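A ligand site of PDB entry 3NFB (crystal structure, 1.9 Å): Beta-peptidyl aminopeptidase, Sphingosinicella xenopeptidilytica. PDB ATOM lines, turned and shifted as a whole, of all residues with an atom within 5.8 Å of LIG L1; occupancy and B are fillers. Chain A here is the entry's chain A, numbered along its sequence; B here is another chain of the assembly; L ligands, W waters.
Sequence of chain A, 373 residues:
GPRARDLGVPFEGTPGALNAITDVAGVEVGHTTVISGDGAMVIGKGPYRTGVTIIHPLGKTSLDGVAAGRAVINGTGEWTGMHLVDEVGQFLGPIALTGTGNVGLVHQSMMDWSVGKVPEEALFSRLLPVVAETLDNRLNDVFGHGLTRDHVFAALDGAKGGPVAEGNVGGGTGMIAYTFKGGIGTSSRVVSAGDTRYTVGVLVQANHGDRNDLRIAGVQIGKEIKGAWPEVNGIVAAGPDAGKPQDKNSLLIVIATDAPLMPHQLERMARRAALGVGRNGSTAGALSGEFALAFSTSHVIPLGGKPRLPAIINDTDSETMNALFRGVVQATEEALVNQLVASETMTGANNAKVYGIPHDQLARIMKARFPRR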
ATOM      1  N   THR A  76      21.121   5.276  -4.328  1.00  0.00           N
ATOM      2  CA  THR A  76      22.168   5.079  -5.343  1.00  0.00           C
ATOM      3  C   THR A  76      22.411   6.358  -6.164  1.00  0.00           C
ATOM      4  O   THR A  76      21.993   6.467  -7.329  1.00  0.00           O
ATOM      5  CB  THR A  76      21.843   3.928  -6.301  1.00  0.00           C
ATOM      6  OG1 THR A  76      20.596   4.177  -6.968  1.00  0.00           O
ATOM      7  CG2 THR A  76      21.773   2.587  -5.559  1.00  0.00           C
ATOM      8  N   GLY A  77      23.103   7.319  -5.560  1.00  0.00           N
ATOM      9  CA  GLY A  77      23.353   8.599  -6.203  1.00  0.00           C
ATOM     10  C   GLY A  77      24.155   9.496  -5.295  1.00  0.00           C
ATOM     11  O   GLY A  77      24.534   9.078  -4.203  1.00  0.00           O
ATOM     12  N   GLU A  78      24.433  10.725  -5.739  1.00  0.00           N
ATOM     13  CA  GLU A  78      25.194  11.669  -4.921  1.00  0.00           C
ATOM     14  C   GLU A  78      24.344  12.903  -4.606  1.00  0.00           C
ATOM     15  O   GLU A  78      23.570  13.387  -5.434  1.00  0.00           O
ATOM     16  CB  GLU A  78      26.510  12.102  -5.601  1.00  0.00           C
ATOM     17  CG  GLU A  78      27.491  12.759  -4.620  1.00  0.00           C
ATOM     18  CD  GLU A  78      27.665  11.911  -3.355  1.00  0.00           C
ATOM     19  OE1 GLU A  78      28.251  10.813  -3.440  1.00  0.00           O
ATOM     20  OE2 GLU A  78      27.173  12.338  -2.287  1.00  0.00           O
ATOM     21  N   THR A 100      25.475  13.681 -13.443  1.00  0.00           N
ATOM     22  CA  THR A 100      26.458  12.999 -12.626  1.00  0.00           C
ATOM     23  C   THR A 100      27.909  13.384 -12.937  1.00  0.00           C
ATOM     24  O   THR A 100      28.737  13.537 -12.046  1.00  0.00           O
ATOM     25  CB  THR A 100      26.322  11.461 -12.778  1.00  0.00           C
ATOM     26  OG1 THR A 100      24.934  11.112 -12.804  1.00  0.00           O
ATOM     27  CG2 THR A 100      27.015  10.727 -11.633  1.00  0.00           C
ATOM     28  N   GLU A 133      22.894  14.906  -8.253  1.00  0.00           N
ATOM     29  CA  GLU A 133      22.927  14.465  -9.645  1.00  0.00           C
ATOM     30  C   GLU A 133      21.908  13.390 -10.032  1.00  0.00           C
ATOM     31  O   GLU A 133      21.440  12.619  -9.186  1.00  0.00           O
ATOM     32  CB  GLU A 133      24.325  13.917 -10.001  1.00  0.00           C
ATOM     33  CG  GLU A 133      24.803  12.725  -9.136  1.00  0.00           C
ATOM     34  CD  GLU A 133      24.130  11.387  -9.446  1.00  0.00           C
ATOM     35  OE1 GLU A 133      24.003  10.574  -8.508  1.00  0.00           O
ATOM     36  OE2 GLU A 133      23.737  11.115 -10.618  1.00  0.00           O
ATOM     37  N   THR A 134      21.553  13.378 -11.315  1.00  0.00           N
ATOM     38  CA  THR A 134      21.011  12.198 -11.984  1.00  0.00           C
ATOM     39  C   THR A 134      21.829  12.007 -13.271  1.00  0.00           C
ATOM     40  O   THR A 134      22.502  12.936 -13.711  1.00  0.00           O
ATOM     41  CB  THR A 134      19.494  12.323 -12.284  1.00  0.00           C
ATOM     42  OG1 THR A 134      19.271  13.344 -13.261  1.00  0.00           O
ATOM     43  CG2 THR A 134      18.713  12.681 -10.997  1.00  0.00           C
ATOM     44  N   LEU A 135      21.779  10.825 -13.871  1.00  0.00           N
ATOM     45  CA  LEU A 135      22.709  10.481 -14.962  1.00  0.00           C
ATOM     46  C   LEU A 135      22.086  10.663 -16.350  1.00  0.00           C
ATOM     47  O   LEU A 135      21.099  10.002 -16.688  1.00  0.00           O
ATOM     48  CB  LEU A 135      23.219   9.053 -14.811  1.00  0.00           C
ATOM     49  CG  LEU A 135      24.260   8.551 -15.829  1.00  0.00           C
ATOM     50  CD1 LEU A 135      25.517   9.416 -15.843  1.00  0.00           C
ATOM     51  CD2 LEU A 135      24.625   7.102 -15.552  1.00  0.00           C
ATOM     52  N   ASN A 137      23.163   9.704 -19.306  1.00  0.00           N
ATOM     53  CA  ASN A 137      24.122   8.913 -20.098  1.00  0.00           C
ATOM     54  C   ASN A 137      23.669   8.519 -21.505  1.00  0.00           C
ATOM     55  O   ASN A 137      24.495   8.186 -22.351  1.00  0.00           O
ATOM     56  CB  ASN A 137      24.520   7.656 -19.354  1.00  0.00           C
ATOM     57  CG  ASN A 137      23.351   6.744 -19.117  1.00  0.00           C
ATOM     58  OD1 ASN A 137      22.336   7.159 -18.545  1.00  0.00           O
ATOM     59  ND2 ASN A 137      23.454   5.504 -19.587  1.00  0.00           N
ATOM     60  N   ASN A 207      14.411  11.624 -13.713  1.00  0.00           N
ATOM     61  CA  ASN A 207      15.190  10.739 -14.570  1.00  0.00           C
ATOM     62  C   ASN A 207      14.846   9.290 -14.215  1.00  0.00           C
ATOM     63  O   ASN A 207      15.696   8.391 -14.273  1.00  0.00           O
ATOM     64  CB  ASN A 207      16.691  11.031 -14.382  1.00  0.00           C
ATOM     65  CG  ASN A 207      17.556  10.362 -15.438  1.00  0.00           C
ATOM     66  OD1 ASN A 207      17.407  10.595 -16.627  1.00  0.00           O
ATOM     67  ND2 ASN A 207      18.502   9.526 -14.991  1.00  0.00           N
ATOM     68  N   HIS A 208      13.587   9.063 -13.854  1.00  0.00           N
ATOM     69  CA  HIS A 208      13.177   7.824 -13.192  1.00  0.00           C
ATOM     70  C   HIS A 208      11.991   7.170 -13.869  1.00  0.00           C
ATOM     71  O   HIS A 208      11.300   7.795 -14.690  1.00  0.00           O
ATOM     72  CB  HIS A 208      12.769   8.147 -11.757  1.00  0.00           C
ATOM     73  CG  HIS A 208      11.481   8.912 -11.674  1.00  0.00           C
ATOM     74  ND1 HIS A 208      11.341  10.165 -12.213  1.00  0.00           N
ATOM     75  CD2 HIS A 208      10.261   8.563 -11.187  1.00  0.00           C
ATOM     76  CE1 HIS A 208      10.096  10.579 -12.035  1.00  0.00           C
ATOM     77  NE2 HIS A 208       9.418   9.628 -11.418  1.00  0.00           N
ATOM     78  N   SER A 250      16.480   7.720 -11.488  1.00  0.00           N
ATOM     79  CA  SER A 250      16.892   8.670 -10.460  1.00  0.00           C
ATOM     80  C   SER A 250      15.965   9.879 -10.441  1.00  0.00           C
ATOM     81  O   SER A 250      15.365  10.223 -11.456  1.00  0.00           O
ATOM     82  CB  SER A 250      18.332   9.143 -10.668  1.00  0.00           C
ATOM     83  OG  SER A 250      19.237   8.061 -10.494  1.00  0.00           O
ATOM     84  N   LEU A 287      19.081   1.001  -9.283  1.00  0.00           N
ATOM     85  CA  LEU A 287      20.144   2.005  -9.458  1.00  0.00           C
ATOM     86  C   LEU A 287      19.584   3.428  -9.613  1.00  0.00           C
ATOM     87  O   LEU A 287      20.297   4.348 -10.022  1.00  0.00           O
ATOM     88  CB  LEU A 287      21.046   1.659 -10.640  1.00  0.00           C
ATOM     89  CG  LEU A 287      21.951   0.429 -10.417  1.00  0.00           C
ATOM     90  CD1 LEU A 287      22.718   0.078 -11.688  1.00  0.00           C
ATOM     91  CD2 LEU A 287      22.918   0.668  -9.258  1.00  0.00           C
ATOM     92  N   SER A 288      18.320   3.596  -9.252  1.00  0.00           N
ATOM     93  CA  SER A 288      17.650   4.882  -9.383  1.00  0.00           C
ATOM     94  C   SER A 288      17.842   5.653  -8.076  1.00  0.00           C
ATOM     95  O   SER A 288      17.232   5.314  -7.072  1.00  0.00           O
ATOM     96  CB  SER A 288      16.160   4.675  -9.678  1.00  0.00           C
ATOM     97  OG  SER A 288      15.439   5.906  -9.731  1.00  0.00           O
ATOM     98  N   GLY A 289      18.693   6.675  -8.094  1.00  0.00           N
ATOM     99  CA  GLY A 289      18.948   7.488  -6.909  1.00  0.00           C
ATOM    100  C   GLY A 289      17.818   8.490  -6.708  1.00  0.00           C
ATOM    101  O   GLY A 289      17.753   9.506  -7.407  1.00  0.00           O
ATOM    102  N   LEU B  84      25.472   5.829  -1.414  1.00  0.00           N
ATOM    103  CA  LEU B  84      25.601   4.536  -2.099  1.00  0.00           C
ATOM    104  C   LEU B  84      25.942   3.427  -1.120  1.00  0.00           C
ATOM    105  O   LEU B  84      25.351   2.341  -1.161  1.00  0.00           O
ATOM    106  CB  LEU B  84      26.706   4.636  -3.173  1.00  0.00           C
ATOM    107  CG  LEU B  84      26.994   3.364  -3.970  1.00  0.00           C
ATOM    108  CD1 LEU B  84      25.824   3.047  -4.919  1.00  0.00           C
ATOM    109  CD2 LEU B  84      28.300   3.533  -4.741  1.00  0.00           C
ATOM    110  N   PHE B 124      30.225   3.783 -16.083  1.00  0.00           N
ATOM    111  CA  PHE B 124      29.180   4.332 -15.217  1.00  0.00           C
ATOM    112  C   PHE B 124      29.437   3.977 -13.750  1.00  0.00           C
ATOM    113  O   PHE B 124      29.024   4.705 -12.842  1.00  0.00           O
ATOM    114  CB  PHE B 124      27.784   3.857 -15.648  1.00  0.00           C
ATOM    115  CG  PHE B 124      27.407   2.521 -15.071  1.00  0.00           C
ATOM    116  CD1 PHE B 124      26.883   2.422 -13.785  1.00  0.00           C
ATOM    117  CD2 PHE B 124      27.566   1.358 -15.809  1.00  0.00           C
ATOM    118  CE1 PHE B 124      26.541   1.185 -13.250  1.00  0.00           C
ATOM    119  CE2 PHE B 124      27.221   0.133 -15.287  1.00  0.00           C
ATOM    120  CZ  PHE B 124      26.710   0.046 -14.001  1.00  0.00           C
ATOM    121  N   SER B 125      30.108   2.852 -13.530  1.00  0.00           N
ATOM    122  CA  SER B 125      30.447   2.390 -12.189  1.00  0.00           C
ATOM    123  C   SER B 125      31.526   3.267 -11.529  1.00  0.00           C
ATOM    124  O   SER B 125      31.831   3.094 -10.354  1.00  0.00           O
ATOM    125  CB  SER B 125      30.932   0.930 -12.224  1.00  0.00           C
ATOM    126  OG  SER B 125      32.273   0.842 -12.676  1.00  0.00           O
ATOM    127  N   LEU B 127      31.326   6.635 -11.495  1.00  0.00           N
ATOM    128  CA  LEU B 127      30.733   7.974 -11.392  1.00  0.00           C
ATOM    129  C   LEU B 127      30.299   8.429  -9.990  1.00  0.00           C
ATOM    130  O   LEU B 127      29.782   9.535  -9.818  1.00  0.00           O
ATOM    131  CB  LEU B 127      29.532   8.087 -12.328  1.00  0.00           C
ATOM    132  CG  LEU B 127      29.865   8.228 -13.806  1.00  0.00           C
ATOM    133  CD1 LEU B 127      28.589   8.036 -14.633  1.00  0.00           C
ATOM    134  CD2 LEU B 127      30.506   9.579 -14.077  1.00  0.00           C
ATOM    135  N   LEU B 128      30.518   7.567  -8.995  1.00  0.00           N
ATOM    136  CA  LEU B 128      30.244   7.932  -7.611  1.00  0.00           C
ATOM    137  C   LEU B 128      31.508   7.791  -6.733  1.00  0.00           C
ATOM    138  O   LEU B 128      31.526   7.032  -5.766  1.00  0.00           O
ATOM    139  CB  LEU B 128      29.068   7.094  -7.058  1.00  0.00           C
ATOM    140  CG  LEU B 128      27.694   7.354  -7.685  1.00  0.00           C
ATOM    141  CD1 LEU B 128      26.611   6.370  -7.178  1.00  0.00           C
ATOM    142  CD2 LEU B 128      27.256   8.796  -7.442  1.00  0.00           C
HETATM  143  O1  LIG L   1      19.030   6.370 -14.954  1.00  0.00           O
HETATM  144  C1  LIG L   1      23.188   3.647 -16.362  1.00  0.00           C
HETATM  145  N1  LIG L   1      21.126   6.020 -12.068  1.00  0.00           N
HETATM  146  O2  LIG L   1      20.333   3.150 -17.592  1.00  0.00           O
HETATM  147  S1  LIG L   1      22.529   3.871 -13.808  1.00  0.00           S
HETATM  148  C2  LIG L   1      20.799   2.308 -16.782  1.00  0.00           C
HETATM  149  N2  LIG L   1      22.334   8.657  -9.782  1.00  0.00           N
HETATM  150  O3  LIG L   1      20.816   1.093 -17.120  1.00  0.00           O
HETATM  151  C3  LIG L   1      21.628   7.271 -11.615  1.00  0.00           C
HETATM  152  N3  LIG L   1      20.282   3.957 -15.103  1.00  0.00           N
HETATM  153  O4  LIG L   1      21.567   8.256 -12.304  1.00  0.00           O
HETATM  154  C4  LIG L   1      22.338   7.276 -10.272  1.00  0.00           C
HETATM  155  O5  LIG L   1      18.800   6.923 -12.882  1.00  0.00           O
HETATM  156  C5  LIG L   1      23.728   6.623 -10.432  1.00  0.00           C
HETATM  157  C6  LIG L   1      22.533   2.918 -15.188  1.00  0.00           C
HETATM  158  C7  LIG L   1      24.775   7.353 -10.970  1.00  0.00           C
HETATM  159  C8  LIG L   1      26.027   6.760 -11.167  1.00  0.00           C
HETATM  160  C9  LIG L   1      26.225   5.426 -10.835  1.00  0.00           C
HETATM  161  C10 LIG L   1      25.164   4.684 -10.297  1.00  0.00           C
HETATM  162  C11 LIG L   1      23.911   5.289 -10.112  1.00  0.00           C
HETATM  163  C12 LIG L   1      21.024   2.628 -15.490  1.00  0.00           C
HETATM  164  C13 LIG L   1      20.967   4.327 -13.690  1.00  0.00           C
HETATM  165  C14 LIG L   1      20.843   5.755 -13.462  1.00  0.00           C
HETATM  166  C15 LIG L   1      19.448   6.279 -13.759  1.00  0.00           C
HETATM  167  C16 LIG L   1      23.243   1.604 -14.950  1.00  0.00           C
HETATM  168  O1  LG2 L   2      12.526   0.587 -21.095  1.00  0.00           O
HETATM  169  C1  LG2 L   2      16.887   3.066 -24.323  1.00  0.00           C
HETATM  170  N1  LG2 L   2      15.182  -0.423 -23.113  1.00  0.00           N
HETATM  171  O2  LG2 L   2      18.844   4.381 -22.046  1.00  0.00           O
HETATM  172  S1  LG2 L   2      14.741   2.462 -22.908  1.00  0.00           S
HETATM  173  C2  LG2 L   2      18.292   3.252 -22.024  1.00  0.00           C
HETATM  174  N2  LG2 L   2      16.940  -3.433 -24.328  1.00  0.00           N
HETATM  175  O3  LG2 L   2      19.014   2.218 -22.006  1.00  0.00           O
HETATM  176  C3  LG2 L   2      16.207  -1.455 -23.158  1.00  0.00           C
HETATM  177  N3  LG2 L   2      16.616   1.675 -21.362  1.00  0.00           N
HETATM  178  O4  LG2 L   2      16.882  -1.675 -22.172  1.00  0.00           O
HETATM  179  C4  LG2 L   2      16.651  -2.008 -24.492  1.00  0.00           C
HETATM  180  O5  LG2 L   2      12.844  -1.276 -22.179  1.00  0.00           O
HETATM  181  C5  LG2 L   2      17.840  -1.236 -25.074  1.00  0.00           C
HETATM  182  C6  LG2 L   2      16.112   3.417 -23.059  1.00  0.00           C
HETATM  183  C7  LG2 L   2      17.932  -1.046 -26.440  1.00  0.00           C
HETATM  184  C8  LG2 L   2      18.996  -0.325 -26.967  1.00  0.00           C
HETATM  185  C9  LG2 L   2      19.975   0.205 -26.120  1.00  0.00           C
HETATM  186  C10 LG2 L   2      19.877   0.003 -24.748  1.00  0.00           C
HETATM  187  C11 LG2 L   2      18.812  -0.708 -24.221  1.00  0.00           C
HETATM  188  C12 LG2 L   2      16.966   3.143 -21.787  1.00  0.00           C
HETATM  189  C13 LG2 L   2      15.036   1.524 -21.614  1.00  0.00           C
HETATM  190  C14 LG2 L   2      14.767   0.107 -21.812  1.00  0.00           C
HETATM  191  C15 LG2 L   2      13.289  -0.195 -21.718  1.00  0.00           C
HETATM  192  C16 LG2 L   2      15.735   4.879 -23.105  1.00  0.00           C
HETATM  193  O   HOH W   1      16.007   5.098 -12.925  1.00  0.00           O
HETATM  194  O   HOH W   2      20.915   4.184 -20.062  1.00  0.00           O
HETATM  195  O   HOH W   3      20.364   6.517 -16.979  1.00  0.00           O
HETATM  196  O   HOH W   4      20.418  10.175  -8.091  1.00  0.00           O
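Water W3 bridges O1 of LIG L1 (2.4 Å) and OD1 of Asn 137 (2.6 Å). Water W2 lies within hydrogen-bond range of O2 of LIG L1 (2.7 Å), O2 of LG2 L2 (2.9 Å) and ND2 of Asn 137 (2.9 Å). Water W4 lies within hydrogen-bond range of O of Gly 289 (2.8 Å), O of Glu 133 (2.9 Å), N2 of LIG L1 (3.0 Å) and OG of Ser 250 (3.4 Å). Water W1 lies within hydrogen-bond range of N of Ser 250 (3.0 Å), O5 of LIG L1 (3.3 Å) and OG of Ser 288 (3.3 Å).
The backbone NH (N) of Ser 250 is in hydrogen-bond range of an oxygen (O5) of LIG L1 (2.8 Å). The side-chain hydroxyl (OG) of Ser 250 lies within hydrogen-bond range of an oxygen (O5) of LIG L1 (2.7 Å). The backbone carbonyl oxygen (O) of Leu 287 lies within hydrogen-bond range of a nitrogen (N1) of LIG L1, at 2.8 Å. OE1 of Glu 133 is in salt-bridge range of N2 of LIG L1 (2.8 Å). N of Leu 135 is in hydrogen-bond range of O4 of LIG L1, 3.0 Å away. O of Thr 76 sits close to N2 of LIG L1 (3.3 Å). An oxygen (O1) of LIG L1 is in hydrogen-bond range of the side-chain amide nitrogen of Asn 207 (3.2 Å).
O of Ser 250 is in hydrogen-bond range of N of Asn 207 (2.8 Å). N of Ser 250 is in hydrogen-bond range of OG of Ser 288 (2.7 Å). The backbone NH (N) of His 208 lies within hydrogen-bond range of the backbone carbonyl oxygen (O) of Ser 250 (3.2 Å). OE2 of Glu 133 is in hydrogen-bond range of OG1 of Thr 100, at 2.5 Å. The backbone carbonyl oxygen (O) of Leu 135 sits at hydrogen-bond distance from the side-chain amide nitrogen (ND2) of Asn 207. OG1 of Thr 76 sits at hydrogen-bond distance from N of Ser 288, 3.3 Å away. OG1 of Thr 76 sits at hydrogen-bond distance from N of Gly 289 (3.3 Å). N of Thr 100 is in hydrogen-bond range of O of Thr 134 (3.1 Å).
Residues that only touch LIG L1: Phe 124 of chain B, Gly 77, Asn 137, Leu 128 of chain B, Thr 134 and Leu 127 of chain B. Hydrophobic or aromatic side chains within 4 Å of LIG L1: Leu 135, Leu 287, Phe 124 of chain B, Leu 127 of chain B and Leu 128 of chain B. Within 4 Å of LIG L1: Thr 76, Gly 77, Glu 133, Thr 134, Leu 135, Asn 137, Asn 207, Ser 250, Leu 287, Phe 124 of chain B, Leu 127 of chain B and Leu 128 of chain B. Along chain A the residues within 4 Å of LIG L1 span positions 76 to 287. The nearest printed residue that does not touch LIG L1 is Thr 100 (4.1 Å).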
